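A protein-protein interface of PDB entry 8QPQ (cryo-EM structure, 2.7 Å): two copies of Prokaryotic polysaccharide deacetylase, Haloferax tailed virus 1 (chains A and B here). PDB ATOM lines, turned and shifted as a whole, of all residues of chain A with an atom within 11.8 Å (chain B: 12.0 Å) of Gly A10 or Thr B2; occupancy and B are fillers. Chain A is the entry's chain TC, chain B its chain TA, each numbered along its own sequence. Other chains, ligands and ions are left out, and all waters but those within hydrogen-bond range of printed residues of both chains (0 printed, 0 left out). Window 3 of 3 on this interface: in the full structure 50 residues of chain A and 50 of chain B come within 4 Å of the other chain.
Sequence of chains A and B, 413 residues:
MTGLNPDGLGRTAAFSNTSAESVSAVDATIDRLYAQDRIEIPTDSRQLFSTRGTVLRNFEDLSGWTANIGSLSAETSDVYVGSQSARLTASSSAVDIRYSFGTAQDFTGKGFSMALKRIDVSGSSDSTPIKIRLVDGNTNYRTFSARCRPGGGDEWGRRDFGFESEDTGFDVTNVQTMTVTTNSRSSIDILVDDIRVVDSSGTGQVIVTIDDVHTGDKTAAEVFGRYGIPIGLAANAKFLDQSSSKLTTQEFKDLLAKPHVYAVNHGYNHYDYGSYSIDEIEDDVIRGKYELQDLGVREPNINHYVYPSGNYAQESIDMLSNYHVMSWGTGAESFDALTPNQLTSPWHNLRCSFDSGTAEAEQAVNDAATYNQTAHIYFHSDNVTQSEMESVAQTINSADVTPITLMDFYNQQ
Ala A13 touches Phe B15, but with the chains exchanged Phe A15 does not touch Ala B13 (6.8 Å).
Phe A15 touches its own counterpart, Phe B15.
Positions printed for both chains: 4, 5, 6, 7, 12, 13, 14 and 15.
Of the 21 pairs that touch across the chains among the printed residues, 1 has its exchanged pair printed and touching as well.
Of the printed residues of chain B, Pro A6 touches Asn B17 (3.6 Å), Thr B18 (3.8 Å) and Ser B19 (3.6 Å).
No residue of chain B comes within 4 Å of Gly A8.
Of the printed residues of chain B, Gly A10 touches Thr B2 and Ser B16.
Printed residues of chain B within 4 Å of Val A26: Asp B31 (3.3 Å).
No residue of chain A comes within 4 Å of Gly B3.
Of the printed residues of chain A, Ala B13 touches Arg A11.
Of chain A, only Arg A11 comes within 4 Å of Ala B14.
Of the printed residues of chain A, Asp B31 touches Ala A25 (3.0 Å) and Val A26 (3.3 Å).
The nearest printed residue of chain A that does not touch Thr B18 is Phe A15 (4.2 Å).
The side-chain amide nitrogen of Asn A5 lies within hydrogen-bond range of the backbone carbonyl oxygen of Thr A12 (3.3 Å).
OD1 of Asn A5 lies within hydrogen-bond range of N of Ala A14 (2.9 Å).
The side-chain hydroxyl of Ser B16 is in hydrogen-bond range of the side-chain hydroxyl of Thr B2, at 2.7 Å.
The side-chain amide oxygen (OD1) of Asn B5 lies within hydrogen-bond range of the backbone NH (N) of Ala B14 (2.9 Å).
Of the 15 printed residues of chain A, 11 touch a printed residue of chain B.
Hydrophobic or aromatic side chains of chain A within 4 Å of the printed part of chain B: Pro A6, Ala A13 and Phe A15.
Printed residues of chain B that touch a printed residue of chain A: Thr B2, Ala B13, Ala B14, Phe B15, Ser B16, Asn B17, Thr B18, Ser B19 and Asp B31.
Hydrophobic or aromatic side chains of chain B that line the printed part of chain A: Ala B13 and Phe B15.
Among the printed residues, 21 pairs touch across the chains.
Among the printed residues, no Asp or Glu carboxylate lies within 4 Å of a Lys or Arg side-chain nitrogen of the other chain.
The backbone carbonyl oxygen (O) of Asp A7 lies within hydrogen-bond range of the side-chain amide nitrogen (ND2) of Asn B17, 2.7 Å away.
The backbone carbonyl oxygen (O) of Leu A9 sits close to the side-chain hydroxyl (OG) of Ser B16 (3.2 Å).
The backbone carbonyl oxygen (O) of Arg A11 is in hydrogen-bond range of the backbone NH (N) of Ser B16.
The backbone NH (N) of Ala A13 sits at hydrogen-bond distance from the backbone carbonyl oxygen (O) of Asn B17, 3.3 Å away.
The backbone NH (N) of Ser B19 sits at hydrogen-bond distance from the backbone carbonyl oxygen (O) of Ala A13 (3.0 Å).
The backbone NH of Phe A15 is in hydrogen-bond range of the backbone carbonyl oxygen of Ser B19.
The backbone carbonyl oxygen of Ala A25 lies within hydrogen-bond range of the backbone NH of Asp B31, at 3.0 Å.
O of Val A26 lies within hydrogen-bond range of N of Asp B31, 3.3 Å away.
Among the printed residues, merely in contact across the chains: Arg A11 with Phe B15 (3.3 Å), Thr A12 with Asn B17 (3.3 Å), Ala A13 with Thr B18 (3.3 Å), Gly A10 with Thr B2 (3.4 Å), Arg A11 with Ala B14 (3.4 Å), Arg A11 with Ala B13 (3.5 Å), Ala A14 with Ser B19 (3.6 Å), Pro A6 with Ser B19 (3.6 Å), Gly A10 with Ser B16 (3.6 Å), Pro A6 with Asn B17 (3.6 Å), Phe A15 with Phe B15 (3.8 Å), Pro A6 with Thr B18 (3.8 Å) and Ala A13 with Phe B15 (3.96 Å).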
ATOM      1  N   LEU A   4     -15.626  20.976  10.854  1.00  0.00           N
ATOM      2  CA  LEU A   4     -15.099  19.616  10.906  1.00  0.00           C
ATOM      3  C   LEU A   4     -13.656  19.588  10.398  1.00  0.00           C
ATOM      4  O   LEU A   4     -13.168  20.559   9.811  1.00  0.00           O
ATOM      5  CB  LEU A   4     -16.004  18.675  10.104  1.00  0.00           C
ATOM      6  CG  LEU A   4     -17.453  18.598  10.581  1.00  0.00           C
ATOM      7  CD1 LEU A   4     -18.277  17.721   9.664  1.00  0.00           C
ATOM      8  CD2 LEU A   4     -17.526  18.103  12.015  1.00  0.00           C
ATOM      9  N   ASN A   5     -12.963  18.471  10.642  1.00  0.00           N
ATOM     10  CA  ASN A   5     -11.545  18.351  10.333  1.00  0.00           C
ATOM     11  C   ASN A   5     -11.294  18.506   8.830  1.00  0.00           C
ATOM     12  O   ASN A   5     -12.099  18.059   8.017  1.00  0.00           O
ATOM     13  CB  ASN A   5     -10.994  17.028  10.856  1.00  0.00           C
ATOM     14  CG  ASN A   5     -10.685  17.037  12.337  1.00  0.00           C
ATOM     15  OD1 ASN A   5     -10.782  18.063  12.996  1.00  0.00           O
ATOM     16  ND2 ASN A   5     -10.320  15.888  12.874  1.00  0.00           N
ATOM     17  N   PRO A   6     -10.182  19.160   8.407  1.00  0.00           N
ATOM     18  CA  PRO A   6      -9.841  19.268   6.989  1.00  0.00           C
ATOM     19  C   PRO A   6      -9.706  17.925   6.286  1.00  0.00           C
ATOM     20  O   PRO A   6      -9.425  16.896   6.899  1.00  0.00           O
ATOM     21  CB  PRO A   6      -8.464  19.947   7.004  1.00  0.00           C
ATOM     22  CG  PRO A   6      -8.469  20.756   8.277  1.00  0.00           C
ATOM     23  CD  PRO A   6      -9.230  19.892   9.262  1.00  0.00           C
ATOM     24  N   ASP A   7      -9.922  17.973   4.976  1.00  0.00           N
ATOM     25  CA  ASP A   7      -9.660  16.894   4.040  1.00  0.00           C
ATOM     26  C   ASP A   7      -8.223  16.399   4.202  1.00  0.00           C
ATOM     27  O   ASP A   7      -7.285  17.190   4.150  1.00  0.00           O
ATOM     28  CB  ASP A   7      -9.940  17.417   2.630  1.00  0.00           C
ATOM     29  CG  ASP A   7      -9.569  16.518   1.458  1.00  0.00           C
ATOM     30  OD1 ASP A   7      -9.074  15.388   1.676  1.00  0.00           O
ATOM     31  OD2 ASP A   7      -9.797  16.953   0.308  1.00  0.00           O
ATOM     32  N   GLY A   8      -8.066  15.083   4.381  1.00  0.00           N
ATOM     33  CA  GLY A   8      -6.767  14.463   4.213  1.00  0.00           C
ATOM     34  C   GLY A   8      -6.545  13.310   5.177  1.00  0.00           C
ATOM     35  O   GLY A   8      -7.190  13.205   6.215  1.00  0.00           O
ATOM     36  N   LEU A   9      -5.586  12.465   4.815  1.00  0.00           N
ATOM     37  CA  LEU A   9      -5.021  11.526   5.761  1.00  0.00           C
ATOM     38  C   LEU A   9      -3.859  12.170   6.517  1.00  0.00           C
ATOM     39  O   LEU A   9      -3.593  13.363   6.351  1.00  0.00           O
ATOM     40  CB  LEU A   9      -4.623  10.273   4.988  1.00  0.00           C
ATOM     41  CG  LEU A   9      -5.796   9.476   4.438  1.00  0.00           C
ATOM     42  CD1 LEU A   9      -5.273   8.227   3.764  1.00  0.00           C
ATOM     43  CD2 LEU A   9      -6.757   9.107   5.555  1.00  0.00           C
ATOM     44  N   GLY A  10      -3.236  11.387   7.402  1.00  0.00           N
ATOM     45  CA  GLY A  10      -2.384  11.924   8.444  1.00  0.00           C
ATOM     46  C   GLY A  10      -3.213  12.587   9.541  1.00  0.00           C
ATOM     47  O   GLY A  10      -4.439  12.671   9.449  1.00  0.00           O
ATOM     48  N   ARG A  11      -2.529  13.081  10.575  1.00  0.00           N
ATOM     49  CA  ARG A  11      -3.172  13.841  11.632  1.00  0.00           C
ATOM     50  C   ARG A  11      -3.730  15.150  11.062  1.00  0.00           C
ATOM     51  O   ARG A  11      -2.985  16.001  10.601  1.00  0.00           O
ATOM     52  CB  ARG A  11      -2.153  14.069  12.750  1.00  0.00           C
ATOM     53  CG  ARG A  11      -2.755  14.505  14.076  1.00  0.00           C
ATOM     54  CD  ARG A  11      -1.680  14.538  15.140  1.00  0.00           C
ATOM     55  NE  ARG A  11      -2.093  15.311  16.300  1.00  0.00           N
ATOM     56  CZ  ARG A  11      -1.363  15.487  17.393  1.00  0.00           C
ATOM     57  NH1 ARG A  11      -1.842  16.215  18.389  1.00  0.00           N
ATOM     58  NH2 ARG A  11      -0.161  14.944  17.501  1.00  0.00           N
ATOM     59  N   THR A  12      -5.060  15.284  11.078  1.00  0.00           N
ATOM     60  CA  THR A  12      -5.748  16.484  10.633  1.00  0.00           C
ATOM     61  C   THR A  12      -6.535  17.044  11.813  1.00  0.00           C
ATOM     62  O   THR A  12      -7.075  16.277  12.622  1.00  0.00           O
ATOM     63  CB  THR A  12      -6.680  16.207   9.445  1.00  0.00           C
ATOM     64  OG1 THR A  12      -7.538  15.106   9.779  1.00  0.00           O
ATOM     65  CG2 THR A  12      -5.923  15.877   8.181  1.00  0.00           C
ATOM     66  N   ALA A  13      -6.612  18.381  11.902  1.00  0.00           N
ATOM     67  CA  ALA A  13      -7.328  18.997  13.008  1.00  0.00           C
ATOM     68  C   ALA A  13      -7.992  20.309  12.598  1.00  0.00           C
ATOM     69  O   ALA A  13      -7.396  21.122  11.900  1.00  0.00           O
ATOM     70  CB  ALA A  13      -6.396  19.204  14.170  1.00  0.00           C
ATOM     71  N   ALA A  14      -9.235  20.498  13.064  1.00  0.00           N
ATOM     72  CA  ALA A  14      -9.903  21.786  13.041  1.00  0.00           C
ATOM     73  C   ALA A  14      -9.811  22.416  14.430  1.00  0.00           C
ATOM     74  O   ALA A  14     -10.306  21.858  15.410  1.00  0.00           O
ATOM     75  CB  ALA A  14     -11.334  21.598  12.595  1.00  0.00           C
ATOM     76  N   PHE A  15      -9.183  23.592  14.489  1.00  0.00           N
ATOM     77  CA  PHE A  15      -9.018  24.339  15.720  1.00  0.00           C
ATOM     78  C   PHE A  15      -9.821  25.629  15.671  1.00  0.00           C
ATOM     79  O   PHE A  15     -10.172  26.141  14.609  1.00  0.00           O
ATOM     80  CB  PHE A  15      -7.551  24.724  15.899  1.00  0.00           C
ATOM     81  CG  PHE A  15      -6.612  23.564  16.099  1.00  0.00           C
ATOM     82  CD1 PHE A  15      -6.520  22.933  17.334  1.00  0.00           C
ATOM     83  CD2 PHE A  15      -5.811  23.111  15.061  1.00  0.00           C
ATOM     84  CE1 PHE A  15      -5.636  21.882  17.531  1.00  0.00           C
ATOM     85  CE2 PHE A  15      -4.916  22.067  15.263  1.00  0.00           C
ATOM     86  CZ  PHE A  15      -4.841  21.443  16.492  1.00  0.00           C
ATOM     87  N   SER A  24       5.908  25.093  11.241  1.00  0.00           N
ATOM     88  CA  SER A  24       6.357  24.734   9.908  1.00  0.00           C
ATOM     89  C   SER A  24       5.131  24.384   9.074  1.00  0.00           C
ATOM     90  O   SER A  24       4.347  23.522   9.462  1.00  0.00           O
ATOM     91  CB  SER A  24       7.319  23.573   9.936  1.00  0.00           C
ATOM     92  OG  SER A  24       8.513  23.924  10.610  1.00  0.00           O
ATOM     93  N   ALA A  25       4.970  25.058   7.931  1.00  0.00           N
ATOM     94  CA  ALA A  25       3.914  24.729   6.990  1.00  0.00           C
ATOM     95  C   ALA A  25       4.511  24.675   5.588  1.00  0.00           C
ATOM     96  O   ALA A  25       5.373  25.485   5.244  1.00  0.00           O
ATOM     97  CB  ALA A  25       2.814  25.757   7.069  1.00  0.00           C
ATOM     98  N   VAL A  26       4.022  23.753   4.749  1.00  0.00           N
ATOM     99  CA  VAL A  26       4.336  23.870   3.334  1.00  0.00           C
ATOM    100  C   VAL A  26       3.437  24.958   2.756  1.00  0.00           C
ATOM    101  O   VAL A  26       3.919  26.028   2.410  1.00  0.00           O
ATOM    102  CB  VAL A  26       4.261  22.534   2.573  1.00  0.00           C
ATOM    103  CG1 VAL A  26       4.687  22.708   1.128  1.00  0.00           C
ATOM    104  CG2 VAL A  26       5.093  21.460   3.249  1.00  0.00           C
ATOM    105  N   THR B   2       3.166  12.905   6.386  1.00  0.00           N
ATOM    106  CA  THR B   2       2.995  13.651   7.663  1.00  0.00           C
ATOM    107  C   THR B   2       4.341  13.780   8.375  1.00  0.00           C
ATOM    108  O   THR B   2       4.656  14.858   8.865  1.00  0.00           O
ATOM    109  CB  THR B   2       1.984  12.958   8.576  1.00  0.00           C
ATOM    110  OG1 THR B   2       0.806  12.732   7.800  1.00  0.00           O
ATOM    111  CG2 THR B   2       1.642  13.781   9.794  1.00  0.00           C
ATOM    112  N   GLY B   3       5.122  12.690   8.405  1.00  0.00           N
ATOM    113  CA  GLY B   3       6.378  12.622   9.144  1.00  0.00           C
ATOM    114  C   GLY B   3       6.173  12.390  10.642  1.00  0.00           C
ATOM    115  O   GLY B   3       5.041  12.188  11.090  1.00  0.00           O
ATOM    116  N   LEU B   4       7.277  12.412  11.399  1.00  0.00           N
ATOM    117  CA  LEU B   4       7.222  12.290  12.852  1.00  0.00           C
ATOM    118  C   LEU B   4       7.155  13.668  13.504  1.00  0.00           C
ATOM    119  O   LEU B   4       7.367  14.685  12.845  1.00  0.00           O
ATOM    120  CB  LEU B   4       8.401  11.456  13.365  1.00  0.00           C
ATOM    121  CG  LEU B   4       8.453  10.021  12.843  1.00  0.00           C
ATOM    122  CD1 LEU B   4       9.663   9.293  13.400  1.00  0.00           C
ATOM    123  CD2 LEU B   4       7.171   9.254  13.167  1.00  0.00           C
ATOM    124  N   ASN B   5       6.832  13.701  14.804  1.00  0.00           N
ATOM    125  CA  ASN B   5       6.596  14.950  15.515  1.00  0.00           C
ATOM    126  C   ASN B   5       7.851  15.827  15.523  1.00  0.00           C
ATOM    127  O   ASN B   5       8.964  15.316  15.614  1.00  0.00           O
ATOM    128  CB  ASN B   5       6.106  14.663  16.933  1.00  0.00           C
ATOM    129  CG  ASN B   5       4.627  14.351  17.013  1.00  0.00           C
ATOM    130  OD1 ASN B   5       3.916  14.371  16.014  1.00  0.00           O
ATOM    131  ND2 ASN B   5       4.154  14.063  18.212  1.00  0.00           N
ATOM    132  N   PRO B   6       7.720  17.173  15.436  1.00  0.00           N
ATOM    133  CA  PRO B   6       8.869  18.067  15.560  1.00  0.00           C
ATOM    134  C   PRO B   6       9.620  17.910  16.877  1.00  0.00           C
ATOM    135  O   PRO B   6       9.065  17.514  17.910  1.00  0.00           O
ATOM    136  CB  PRO B   6       8.253  19.472  15.510  1.00  0.00           C
ATOM    137  CG  PRO B   6       6.943  19.290  14.769  1.00  0.00           C
ATOM    138  CD  PRO B   6       6.475  17.907  15.172  1.00  0.00           C
ATOM    139  N   ASP B   7      10.905  18.242  16.794  1.00  0.00           N
ATOM    140  CA  ASP B   7      11.806  18.393  17.922  1.00  0.00           C
ATOM    141  C   ASP B   7      11.197  19.345  18.951  1.00  0.00           C
ATOM    142  O   ASP B   7      10.796  20.454  18.604  1.00  0.00           O
ATOM    143  CB  ASP B   7      13.146  18.902  17.382  1.00  0.00           C
ATOM    144  CG  ASP B   7      14.195  19.354  18.391  1.00  0.00           C
ATOM    145  OD1 ASP B   7      13.971  19.197  19.611  1.00  0.00           O
ATOM    146  OD2 ASP B   7      15.235  19.871  17.942  1.00  0.00           O
ATOM    147  N   THR B  12       3.934  18.952  20.968  1.00  0.00           N
ATOM    148  CA  THR B  12       4.401  19.031  19.589  1.00  0.00           C
ATOM    149  C   THR B  12       3.541  18.105  18.743  1.00  0.00           C
ATOM    150  O   THR B  12       3.062  17.080  19.227  1.00  0.00           O
ATOM    151  CB  THR B  12       5.912  18.782  19.421  1.00  0.00           C
ATOM    152  OG1 THR B  12       6.284  17.422  19.631  1.00  0.00           O
ATOM    153  CG2 THR B  12       6.768  19.682  20.279  1.00  0.00           C
ATOM    154  N   ALA B  13       3.345  18.469  17.471  1.00  0.00           N
ATOM    155  CA  ALA B  13       2.504  17.671  16.592  1.00  0.00           C
ATOM    156  C   ALA B  13       2.963  17.781  15.141  1.00  0.00           C
ATOM    157  O   ALA B  13       3.297  18.869  14.665  1.00  0.00           O
ATOM    158  CB  ALA B  13       1.064  18.103  16.724  1.00  0.00           C
ATOM    159  N   ALA B  14       2.964  16.631  14.450  1.00  0.00           N
ATOM    160  CA  ALA B  14       3.063  16.589  13.001  1.00  0.00           C
ATOM    161  C   ALA B  14       1.665  16.399  12.417  1.00  0.00           C
ATOM    162  O   ALA B  14       1.003  15.390  12.667  1.00  0.00           O
ATOM    163  CB  ALA B  14       4.004  15.489  12.586  1.00  0.00           C
ATOM    164  N   PHE B  15       1.232  17.399  11.641  1.00  0.00           N
ATOM    165  CA  PHE B  15      -0.054  17.382  10.983  1.00  0.00           C
ATOM    166  C   PHE B  15       0.127  17.236   9.481  1.00  0.00           C
ATOM    167  O   PHE B  15       1.173  17.536   8.911  1.00  0.00           O
ATOM    168  CB  PHE B  15      -0.792  18.690  11.236  1.00  0.00           C
ATOM    169  CG  PHE B  15      -1.149  18.945  12.678  1.00  0.00           C
ATOM    170  CD1 PHE B  15      -2.202  18.274  13.288  1.00  0.00           C
ATOM    171  CD2 PHE B  15      -0.447  19.885  13.420  1.00  0.00           C
ATOM    172  CE1 PHE B  15      -2.525  18.519  14.617  1.00  0.00           C
ATOM    173  CE2 PHE B  15      -0.803  20.160  14.736  1.00  0.00           C
ATOM    174  CZ  PHE B  15      -1.859  19.492  15.322  1.00  0.00           C
ATOM    175  N   SER B  16      -0.944  16.770   8.840  1.00  0.00           N
ATOM    176  CA  SER B  16      -1.096  17.000   7.421  1.00  0.00           C
ATOM    177  C   SER B  16      -1.793  18.340   7.230  1.00  0.00           C
ATOM    178  O   SER B  16      -1.120  19.360   7.106  1.00  0.00           O
ATOM    179  CB  SER B  16      -1.731  15.819   6.761  1.00  0.00           C
ATOM    180  OG  SER B  16      -0.773  14.760   6.869  1.00  0.00           O
ATOM    181  N   ASN B  17      -3.127  18.346   7.309  1.00  0.00           N
ATOM    182  CA  ASN B  17      -3.888  19.564   7.052  1.00  0.00           C
ATOM    183  C   ASN B  17      -4.523  20.074   8.343  1.00  0.00           C
ATOM    184  O   ASN B  17      -5.212  19.322   9.026  1.00  0.00           O
ATOM    185  CB  ASN B  17      -4.839  19.373   5.863  1.00  0.00           C
ATOM    186  CG  ASN B  17      -4.123  18.867   4.625  1.00  0.00           C
ATOM    187  OD1 ASN B  17      -2.935  19.135   4.422  1.00  0.00           O
ATOM    188  ND2 ASN B  17      -4.825  18.113   3.795  1.00  0.00           N
ATOM    189  N   THR B  18      -4.310  21.361   8.653  1.00  0.00           N
ATOM    190  CA  THR B  18      -4.951  21.996   9.797  1.00  0.00           C
ATOM    191  C   THR B  18      -5.782  23.198   9.363  1.00  0.00           C
ATOM    192  O   THR B  18      -5.471  23.876   8.391  1.00  0.00           O
ATOM    193  CB  THR B  18      -3.958  22.400  10.895  1.00  0.00           C
ATOM    194  OG1 THR B  18      -3.064  23.411  10.434  1.00  0.00           O
ATOM    195  CG2 THR B  18      -3.216  21.217  11.472  1.00  0.00           C
ATOM    196  N   SER B  19      -6.857  23.432  10.109  1.00  0.00           N
ATOM    197  CA  SER B  19      -7.694  24.610   9.984  1.00  0.00           C
ATOM    198  C   SER B  19      -7.737  25.283  11.351  1.00  0.00           C
ATOM    199  O   SER B  19      -7.810  24.598  12.367  1.00  0.00           O
ATOM    200  CB  SER B  19      -9.074  24.219   9.511  1.00  0.00           C
ATOM    201  OG  SER B  19      -9.966  25.320   9.567  1.00  0.00           O
ATOM    202  N   ASP B  31       6.670  27.467   3.450  1.00  0.00           N
ATOM    203  CA  ASP B  31       7.314  27.205   2.169  1.00  0.00           C
ATOM    204  C   ASP B  31       6.592  27.883   1.001  1.00  0.00           C
ATOM    205  O   ASP B  31       7.216  28.200  -0.014  1.00  0.00           O
ATOM    206  CB  ASP B  31       7.475  25.702   1.936  1.00  0.00           C
ATOM    207  CG  ASP B  31       8.460  25.038   2.886  1.00  0.00           C
ATOM    208  OD1 ASP B  31       9.242  25.765   3.544  1.00  0.00           O
ATOM    209  OD2 ASP B  31       8.453  23.785   2.955  1.00  0.00           O
